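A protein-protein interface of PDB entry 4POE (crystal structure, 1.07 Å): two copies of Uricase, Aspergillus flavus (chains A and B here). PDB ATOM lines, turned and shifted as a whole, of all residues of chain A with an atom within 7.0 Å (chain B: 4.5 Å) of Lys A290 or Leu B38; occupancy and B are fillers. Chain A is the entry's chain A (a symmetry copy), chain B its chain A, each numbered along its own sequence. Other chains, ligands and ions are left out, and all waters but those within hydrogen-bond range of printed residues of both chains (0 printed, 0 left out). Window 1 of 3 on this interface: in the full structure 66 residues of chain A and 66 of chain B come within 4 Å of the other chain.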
ATOM      1  N   ASP A 184     -21.647  27.347 -23.265  1.00  0.00           N
ATOM      2  CA  ASP A 184     -20.952  28.167 -22.296  1.00  0.00           C
ATOM      3  C   ASP A 184     -20.022  27.211 -21.541  1.00  0.00           C
ATOM      4  O   ASP A 184     -20.518  26.386 -20.751  1.00  0.00           O
ATOM      5  CB  ASP A 184     -21.941  28.873 -21.366  1.00  0.00           C
ATOM      6  CG  ASP A 184     -21.376  29.861 -20.386  1.00  0.00           C
ATOM      7  OD1 ASP A 184     -20.126  29.790 -20.233  1.00  0.00           O
ATOM      8  OD2 ASP A 184     -22.119  30.689 -19.809  1.00  0.00           O
ATOM      9  N   VAL A 228     -27.587  15.152 -22.662  1.00  0.00           N
ATOM     10  CA  VAL A 228     -26.676  16.318 -22.594  1.00  0.00           C
ATOM     11  C   VAL A 228     -25.673  16.134 -21.466  1.00  0.00           C
ATOM     12  O   VAL A 228     -24.469  16.421 -21.634  1.00  0.00           O
ATOM     13  CB  VAL A 228     -27.486  17.600 -22.446  1.00  0.00           C
ATOM     14  CG1 VAL A 228     -26.550  18.809 -22.304  1.00  0.00           C
ATOM     15  CG2 VAL A 228     -28.405  17.825 -23.627  1.00  0.00           C
ATOM     16  N   GLN A 229     -26.164  15.638 -20.327  1.00  0.00           N
ATOM     17  CA  GLN A 229     -25.316  15.344 -19.172  1.00  0.00           C
ATOM     18  C   GLN A 229     -24.093  14.536 -19.554  1.00  0.00           C
ATOM     19  O   GLN A 229     -22.933  14.830 -19.207  1.00  0.00           O
ATOM     20  CB  GLN A 229     -26.129  14.600 -18.121  1.00  0.00           C
ATOM     21  CG  GLN A 229     -27.212  15.345 -17.405  1.00  0.00           C
ATOM     22  CD  GLN A 229     -28.581  15.479 -18.110  1.00  0.00           C
ATOM     23  OE1 GLN A 229     -28.668  15.317 -19.324  1.00  0.00           O
ATOM     24  NE2 GLN A 229     -29.581  15.782 -17.362  1.00  0.00           N
ATOM     25  N   MET A 232     -21.613  16.355 -22.185  1.00  0.00           N
ATOM     26  CA  MET A 232     -20.844  17.469 -21.643  1.00  0.00           C
ATOM     27  C   MET A 232     -19.766  16.953 -20.703  1.00  0.00           C
ATOM     28  O   MET A 232     -18.663  17.530 -20.626  1.00  0.00           O
ATOM     29  CB  MET A 232     -21.746  18.510 -20.979  1.00  0.00           C
ATOM     30  CG  MET A 232     -22.360  18.038 -19.658  1.00  0.00           C
ATOM     31  SD  MET A 232     -23.910  18.827 -19.181  1.00  0.00           S
ATOM     32  CE  MET A 232     -23.427  20.527 -19.114  1.00  0.00           C
ATOM     33  N   GLU A 250     -16.326  23.809 -16.226  1.00  0.00           N
ATOM     34  CA  GLU A 250     -17.766  23.991 -16.033  1.00  0.00           C
ATOM     35  C   GLU A 250     -18.416  24.087 -17.394  1.00  0.00           C
ATOM     36  O   GLU A 250     -17.946  24.821 -18.259  1.00  0.00           O
ATOM     37  CB  GLU A 250     -18.114  25.278 -15.269  1.00  0.00           C
ATOM     38  CG  GLU A 250     -17.516  25.537 -13.927  1.00  0.00           C
ATOM     39  CD  GLU A 250     -17.682  26.967 -13.437  1.00  0.00           C
ATOM     40  OE1 GLU A 250     -18.657  27.632 -13.874  1.00  0.00           O
ATOM     41  OE2 GLU A 250     -16.828  27.368 -12.616  1.00  0.00           O
ATOM     42  N   TYR A 251     -19.528  23.392 -17.590  1.00  0.00           N
ATOM     43  CA  TYR A 251     -20.399  23.599 -18.747  1.00  0.00           C
ATOM     44  C   TYR A 251     -21.786  24.008 -18.279  1.00  0.00           C
ATOM     45  O   TYR A 251     -22.311  23.483 -17.293  1.00  0.00           O
ATOM     46  CB  TYR A 251     -20.528  22.323 -19.621  1.00  0.00           C
ATOM     47  CG  TYR A 251     -19.388  22.145 -20.611  1.00  0.00           C
ATOM     48  CD1 TYR A 251     -19.487  22.609 -21.907  1.00  0.00           C
ATOM     49  CD2 TYR A 251     -18.201  21.508 -20.287  1.00  0.00           C
ATOM     50  CE1 TYR A 251     -18.480  22.470 -22.835  1.00  0.00           C
ATOM     51  CE2 TYR A 251     -17.196  21.370 -21.190  1.00  0.00           C
ATOM     52  CZ  TYR A 251     -17.305  21.847 -22.490  1.00  0.00           C
ATOM     53  OH  TYR A 251     -16.270  21.660 -23.325  1.00  0.00           O
ATOM     54  N   SER A 252     -22.376  24.916 -19.063  1.00  0.00           N
ATOM     55  CA  SER A 252     -23.775  25.256 -18.926  1.00  0.00           C
ATOM     56  C   SER A 252     -24.390  25.249 -20.329  1.00  0.00           C
ATOM     57  O   SER A 252     -24.006  26.029 -21.171  1.00  0.00           O
ATOM     58  CB  SER A 252     -23.909  26.614 -18.304  1.00  0.00           C
ATOM     59  OG  SER A 252     -25.263  26.998 -18.139  1.00  0.00           O
ATOM     60  N   LEU A 253     -25.313  24.279 -20.527  1.00  0.00           N
ATOM     61  CA  LEU A 253     -25.840  24.007 -21.843  1.00  0.00           C
ATOM     62  C   LEU A 253     -27.360  24.007 -21.825  1.00  0.00           C
ATOM     63  O   LEU A 253     -28.009  23.153 -21.173  1.00  0.00           O
ATOM     64  CB  LEU A 253     -25.405  22.627 -22.336  1.00  0.00           C
ATOM     65  CG  LEU A 253     -23.878  22.483 -22.524  1.00  0.00           C
ATOM     66  CD1 LEU A 253     -23.537  21.116 -23.038  1.00  0.00           C
ATOM     67  CD2 LEU A 253     -23.307  23.514 -23.512  1.00  0.00           C
ATOM     68  N   GLY A 287     -34.507  23.019 -21.754  1.00  0.00           N
ATOM     69  CA  GLY A 287     -33.697  22.396 -20.703  1.00  0.00           C
ATOM     70  C   GLY A 287     -32.484  23.234 -20.447  1.00  0.00           C
ATOM     71  O   GLY A 287     -31.982  23.947 -21.329  1.00  0.00           O
ATOM     72  N   LEU A 288     -31.964  23.116 -19.216  1.00  0.00           N
ATOM     73  CA  LEU A 288     -30.732  23.807 -18.837  1.00  0.00           C
ATOM     74  C   LEU A 288     -29.953  22.815 -17.990  1.00  0.00           C
ATOM     75  O   LEU A 288     -30.451  22.391 -16.919  1.00  0.00           O
ATOM     76  CB  LEU A 288     -31.031  25.116 -18.128  1.00  0.00           C
ATOM     77  CG  LEU A 288     -29.793  25.869 -17.623  1.00  0.00           C
ATOM     78  CD1 LEU A 288     -28.817  26.182 -18.769  1.00  0.00           C
ATOM     79  CD2 LEU A 288     -30.195  27.138 -16.908  1.00  0.00           C
ATOM     80  N   ILE A 289     -28.767  22.430 -18.455  1.00  0.00           N
ATOM     81  CA  ILE A 289     -27.973  21.361 -17.854  1.00  0.00           C
ATOM     82  C   ILE A 289     -26.629  21.933 -17.489  1.00  0.00           C
ATOM     83  O   ILE A 289     -25.952  22.549 -18.326  1.00  0.00           O
ATOM     84  CB  ILE A 289     -27.838  20.175 -18.837  1.00  0.00           C
ATOM     85  CG1 ILE A 289     -29.143  19.846 -19.561  1.00  0.00           C
ATOM     86  CG2 ILE A 289     -27.211  18.978 -18.147  1.00  0.00           C
ATOM     87  CD1 ILE A 289     -30.335  19.442 -18.762  1.00  0.00           C
ATOM     88  N   LYS A 290     -26.190  21.678 -16.242  1.00  0.00           N
ATOM     89  CA  LYS A 290     -24.935  22.269 -15.754  1.00  0.00           C
ATOM     90  C   LYS A 290     -24.099  21.191 -15.051  1.00  0.00           C
ATOM     91  O   LYS A 290     -24.642  20.277 -14.365  1.00  0.00           O
ATOM     92  CB  LYS A 290     -25.164  23.395 -14.755  1.00  0.00           C
ATOM     93  CG  LYS A 290     -25.943  24.559 -15.349  1.00  0.00           C
ATOM     94  CD  LYS A 290     -26.189  25.670 -14.336  1.00  0.00           C
ATOM     95  CE  LYS A 290     -27.099  26.778 -14.845  1.00  0.00           C
ATOM     96  NZ  LYS A 290     -26.231  27.724 -15.637  1.00  0.00           N
ATOM     97  N   CYS A 291     -22.781  21.310 -15.152  1.00  0.00           N
ATOM     98  CA  CYS A 291     -21.919  20.541 -14.256  1.00  0.00           C
ATOM     99  C   CYS A 291     -20.569  21.250 -14.163  1.00  0.00           C
ATOM    100  O   CYS A 291     -20.132  21.947 -15.075  1.00  0.00           O
ATOM    101  CB  CYS A 291     -21.765  19.136 -14.659  1.00  0.00           C
ATOM    102  SG  CYS A 291     -20.737  17.757 -14.555  1.00  0.00           S
ATOM    103  N   THR A 292     -19.919  20.987 -13.049  1.00  0.00           N
ATOM    104  CA  THR A 292     -18.523  21.317 -12.766  1.00  0.00           C
ATOM    105  C   THR A 292     -17.754  20.022 -12.508  1.00  0.00           C
ATOM    106  O   THR A 292     -18.160  19.233 -11.637  1.00  0.00           O
ATOM    107  CB  THR A 292     -18.376  22.206 -11.533  1.00  0.00           C
ATOM    108  OG1 THR A 292     -19.105  23.445 -11.790  1.00  0.00           O
ATOM    109  CG2 THR A 292     -16.961  22.680 -11.249  1.00  0.00           C
ATOM    110  N   ALA B   7     -23.368  19.599  -9.840  1.00  0.00           N
ATOM    111  CA  ALA B   7     -24.255  19.337 -10.974  1.00  0.00           C
ATOM    112  C   ALA B   7     -25.636  19.824 -10.617  1.00  0.00           C
ATOM    113  O   ALA B   7     -26.098  19.593  -9.497  1.00  0.00           O
ATOM    114  CB  ALA B   7     -24.262  17.878 -11.357  1.00  0.00           C
ATOM    115  N   ARG B   8     -26.291  20.501 -11.556  1.00  0.00           N
ATOM    116  CA  ARG B   8     -27.711  20.843 -11.409  1.00  0.00           C
ATOM    117  C   ARG B   8     -28.308  20.919 -12.804  1.00  0.00           C
ATOM    118  O   ARG B   8     -27.599  21.208 -13.759  1.00  0.00           O
ATOM    119  CB  ARG B   8     -27.971  22.089 -10.608  1.00  0.00           C
ATOM    120  CG  ARG B   8     -27.491  23.385 -11.192  1.00  0.00           C
ATOM    121  CD  ARG B   8     -27.780  24.582 -10.314  1.00  0.00           C
ATOM    122  NE  ARG B   8     -27.041  24.491  -9.071  1.00  0.00           N
ATOM    123  CZ  ARG B   8     -27.130  25.380  -8.107  1.00  0.00           C
ATOM    124  NH1 ARG B   8     -27.907  26.411  -8.077  1.00  0.00           N
ATOM    125  NH2 ARG B   8     -26.365  25.199  -7.015  1.00  0.00           N
ATOM    126  N   TYR B   9     -29.596  20.606 -12.916  1.00  0.00           N
ATOM    127  CA  TYR B   9     -30.206  20.563 -14.230  1.00  0.00           C
ATOM    128  C   TYR B   9     -31.708  20.784 -14.032  1.00  0.00           C
ATOM    129  O   TYR B   9     -32.304  20.486 -13.021  1.00  0.00           O
ATOM    130  CB  TYR B   9     -29.834  19.223 -15.013  1.00  0.00           C
ATOM    131  CG  TYR B   9     -30.816  18.196 -14.516  1.00  0.00           C
ATOM    132  CD1 TYR B   9     -30.717  17.611 -13.237  1.00  0.00           C
ATOM    133  CD2 TYR B   9     -31.941  17.857 -15.322  1.00  0.00           C
ATOM    134  CE1 TYR B   9     -31.656  16.703 -12.778  1.00  0.00           C
ATOM    135  CE2 TYR B   9     -32.898  17.019 -14.833  1.00  0.00           C
ATOM    136  CZ  TYR B   9     -32.748  16.437 -13.604  1.00  0.00           C
ATOM    137  OH  TYR B   9     -33.719  15.569 -13.094  1.00  0.00           O
ATOM    138  N   GLY B  10     -32.374  21.223 -15.118  1.00  0.00           N
ATOM    139  CA  GLY B  10     -33.802  21.374 -15.065  1.00  0.00           C
ATOM    140  C   GLY B  10     -34.342  22.112 -16.248  1.00  0.00           C
ATOM    141  O   GLY B  10     -33.816  22.029 -17.366  1.00  0.00           O
ATOM    142  N   LYS B  11     -35.449  22.838 -16.049  1.00  0.00           N
ATOM    143  CA  LYS B  11     -36.134  23.550 -17.131  1.00  0.00           C
ATOM    144  C   LYS B  11     -36.094  25.047 -16.825  1.00  0.00           C
ATOM    145  O   LYS B  11     -36.472  25.454 -15.731  1.00  0.00           O
ATOM    146  CB  LYS B  11     -37.546  23.080 -17.367  1.00  0.00           C
ATOM    147  CG  LYS B  11     -38.106  23.479 -18.736  1.00  0.00           C
ATOM    148  CD  LYS B  11     -37.528  22.680 -19.856  1.00  0.00           C
ATOM    149  CE  LYS B  11     -38.456  21.707 -20.526  1.00  0.00           C
ATOM    150  NZ  LYS B  11     -37.722  20.754 -21.381  1.00  0.00           N
ATOM    151  N   CYS B  36     -37.793  29.085 -13.634  1.00  0.00           N
ATOM    152  CA  CYS B  36     -36.698  28.143 -13.828  1.00  0.00           C
ATOM    153  C   CYS B  36     -36.613  27.259 -12.597  1.00  0.00           C
ATOM    154  O   CYS B  36     -36.630  27.763 -11.471  1.00  0.00           O
ATOM    155  CB  CYS B  36     -35.388  28.897 -14.018  1.00  0.00           C
ATOM    156  SG  CYS B  36     -33.967  27.779 -14.268  1.00  0.00           S
ATOM    157  N   VAL B  37     -36.537  25.951 -12.790  1.00  0.00           N
ATOM    158  CA  VAL B  37     -36.285  25.003 -11.710  1.00  0.00           C
ATOM    159  C   VAL B  37     -35.092  24.148 -12.082  1.00  0.00           C
ATOM    160  O   VAL B  37     -35.110  23.478 -13.128  1.00  0.00           O
ATOM    161  CB  VAL B  37     -37.508  24.097 -11.449  1.00  0.00           C
ATOM    162  CG1 VAL B  37     -37.127  23.004 -10.431  1.00  0.00           C
ATOM    163  CG2 VAL B  37     -38.736  24.882 -11.026  1.00  0.00           C
ATOM    164  N   LEU B  38     -34.075  24.167 -11.230  1.00  0.00           N
ATOM    165  CA  LEU B  38     -32.904  23.302 -11.369  1.00  0.00           C
ATOM    166  C   LEU B  38     -32.764  22.441 -10.126  1.00  0.00           C
ATOM    167  O   LEU B  38     -32.866  22.924  -9.016  1.00  0.00           O
ATOM    168  CB  LEU B  38     -31.604  24.094 -11.585  1.00  0.00           C
ATOM    169  CG  LEU B  38     -31.634  25.131 -12.705  1.00  0.00           C
ATOM    170  CD1 LEU B  38     -30.332  25.927 -12.707  1.00  0.00           C
ATOM    171  CD2 LEU B  38     -31.943  24.550 -14.049  1.00  0.00           C
ATOM    172  N   LEU B  39     -32.577  21.166 -10.334  1.00  0.00           N
ATOM    173  CA  LEU B  39     -32.439  20.158  -9.311  1.00  0.00           C
ATOM    174  C   LEU B  39     -31.015  19.683  -9.103  1.00  0.00           C
ATOM    175  O   LEU B  39     -30.234  19.602 -10.036  1.00  0.00           O
ATOM    176  CB  LEU B  39     -33.313  18.914  -9.697  1.00  0.00           C
ATOM    177  CG  LEU B  39     -34.783  19.204  -9.978  1.00  0.00           C
ATOM    178  CD1 LEU B  39     -35.512  17.869 -10.251  1.00  0.00           C
ATOM    179  CD2 LEU B  39     -35.458  19.989  -8.899  1.00  0.00           C
ATOM    180  N   GLU B  40     -30.704  19.320  -7.840  1.00  0.00           N
ATOM    181  CA  GLU B  40     -29.483  18.658  -7.475  1.00  0.00           C
ATOM    182  C   GLU B  40     -29.798  17.404  -6.678  1.00  0.00           C
ATOM    183  O   GLU B  40     -30.823  17.351  -5.995  1.00  0.00           O
ATOM    184  CB  GLU B  40     -28.597  19.449  -6.463  1.00  0.00           C
ATOM    185  CG  GLU B  40     -28.118  20.817  -7.002  1.00  0.00           C
ATOM    186  CD  GLU B  40     -27.212  21.434  -5.954  1.00  0.00           C
ATOM    187  OE1 GLU B  40     -26.070  20.915  -5.705  1.00  0.00           O
ATOM    188  OE2 GLU B  40     -27.635  22.378  -5.290  1.00  0.00           O
ATOM    189  N   TYR B  47     -24.251  11.823 -15.656  1.00  0.00           N
ATOM    190  CA  TYR B  47     -23.119  12.423 -16.335  1.00  0.00           C
ATOM    191  C   TYR B  47     -22.032  11.419 -16.644  1.00  0.00           C
ATOM    192  O   TYR B  47     -21.407  11.500 -17.710  1.00  0.00           O
ATOM    193  CB  TYR B  47     -22.556  13.566 -15.458  1.00  0.00           C
ATOM    194  CG  TYR B  47     -23.497  14.712 -15.239  1.00  0.00           C
ATOM    195  CD1 TYR B  47     -24.453  14.708 -14.258  1.00  0.00           C
ATOM    196  CD2 TYR B  47     -23.466  15.918 -16.015  1.00  0.00           C
ATOM    197  CE1 TYR B  47     -25.328  15.725 -14.024  1.00  0.00           C
ATOM    198  CE2 TYR B  47     -24.320  16.957 -15.777  1.00  0.00           C
ATOM    199  CZ  TYR B  47     -25.247  16.912 -14.809  1.00  0.00           C
ATOM    200  OH  TYR B  47     -26.136  17.895 -14.501  1.00  0.00           O
ATOM    201  N   ALA B  97     -31.909  18.991  -3.530  1.00  0.00           N
ATOM    202  CA  ALA B  97     -32.085  20.441  -3.552  1.00  0.00           C
ATOM    203  C   ALA B  97     -32.885  20.837  -4.790  1.00  0.00           C
ATOM    204  O   ALA B  97     -32.743  20.198  -5.857  1.00  0.00           O
ATOM    205  CB  ALA B  97     -30.769  21.207  -3.530  1.00  0.00           C
ATOM    206  N   ALA B  98     -33.681  21.867  -4.655  1.00  0.00           N
ATOM    207  CA  ALA B  98     -34.421  22.452  -5.772  1.00  0.00           C
ATOM    208  C   ALA B  98     -34.180  23.963  -5.714  1.00  0.00           C
ATOM    209  O   ALA B  98     -34.403  24.596  -4.683  1.00  0.00           O
ATOM    210  CB  ALA B  98     -35.881  22.096  -5.672  1.00  0.00           C
ATOM    211  N   HIS B  99     -33.786  24.480  -6.874  1.00  0.00           N
ATOM    212  CA  HIS B  99     -33.458  25.880  -6.997  1.00  0.00           C
ATOM    213  C   HIS B  99     -34.474  26.520  -7.925  1.00  0.00           C
ATOM    214  O   HIS B  99     -34.481  26.219  -9.130  1.00  0.00           O
ATOM    215  CB  HIS B  99     -32.036  26.033  -7.572  1.00  0.00           C
ATOM    216  CG  HIS B  99     -31.013  25.322  -6.772  1.00  0.00           C
ATOM    217  ND1 HIS B  99     -30.604  25.875  -5.534  1.00  0.00           N
ATOM    218  CD2 HIS B  99     -30.369  24.168  -6.955  1.00  0.00           C
ATOM    219  CE1 HIS B  99     -29.684  24.989  -5.071  1.00  0.00           C
ATOM    220  NE2 HIS B  99     -29.528  23.977  -5.862  1.00  0.00           N
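N of Lys A290 is in hydrogen-bond range of O of Arg B8, 2.9 Å away. The backbone carbonyl oxygen (O) of Lys A290 lies within hydrogen-bond range of the side-chain hydroxyl (OH) of Tyr B47. The backbone carbonyl oxygen (O) of Gly B10 sits at hydrogen-bond distance from the backbone NH (N) of Leu A288.
N of Tyr A251 sits at hydrogen-bond distance from O of Cys A291, 3.0 Å away. NZ of Lys A290 lies within hydrogen-bond range of OG of Ser A252, 2.8 Å away. The backbone carbonyl oxygen (O) of Lys B11 lies close to the side-chain sulfur (SG) of Cys B36 (3.7 Å). The backbone carbonyl oxygen (O) of Tyr B9 is in hydrogen-bond range of the backbone NH (N) of Leu B39 (2.8 Å). O of Lys B11 lies within hydrogen-bond range of N of Val B37, at 3.0 Å. NH2 of Arg B8 is in salt-bridge range of OE2 of Glu B40.
CE2 of Tyr B47 touches SD of Met A232 (3.9 Å). CA of Gly A287 touches O of Gly B10 (3.4 Å). N of Gly A287 touches CD of Lys B11 (3.6 Å). Tyr B9 touches Leu A288 (CA to O, 3.3 Å). Leu A288 touches Leu B38 (O to CD2, 3.9 Å). Ile A289 touches Arg B8 (C to O, 3.9 Å). CG2 of Ile A289 touches OH of Tyr B47, 3.95 Å away. Ala B7 touches Lys A290. Lys A290 touches Leu B38. Cys A291 touches Tyr B47.
Lys A290 touches just these residues of chain B: Ala B7, Arg B8, Leu B38 and Tyr B47. Leu B38 touches just these residues of chain A: Leu A288 (3.9 Å) and Lys A290 (3.97 Å). Of the printed residues of chain B, Gln A229 touches Tyr B9 and Tyr B47. Printed residues of chain A within 4 Å of Tyr B9: Gln A229, Leu A288 and Ile A289. Printed residues of chain A within 4 Å of Arg B8: Ile A289 and Lys A290. Printed residues of chain A within 4 Å of Gly B10: Gly A287 (3.4 Å) and Leu A288 (2.8 Å). Of the printed residues of chain A, Ala B7 touches Lys A290. The nearest printed residue of chain B that does not touch Lys A290 is Tyr B9 (4.6 Å).
Of the 14 printed residues of chain B, 7 touch a printed residue of chain A. Hydrophobic or aromatic side chains of chain B that line the printed part of chain A: Ala B7, Tyr B9, Leu B38 and Tyr B47. Along chain A the printed residues that touch a printed residue of chain B span positions 229 to 291. Among the printed residues, 16 pairs touch across the chains. Among the printed residues, no Asp or Glu carboxylate lies within 4 Å of a Lys or Arg side-chain nitrogen of the other chain.
No position is printed for both chains.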
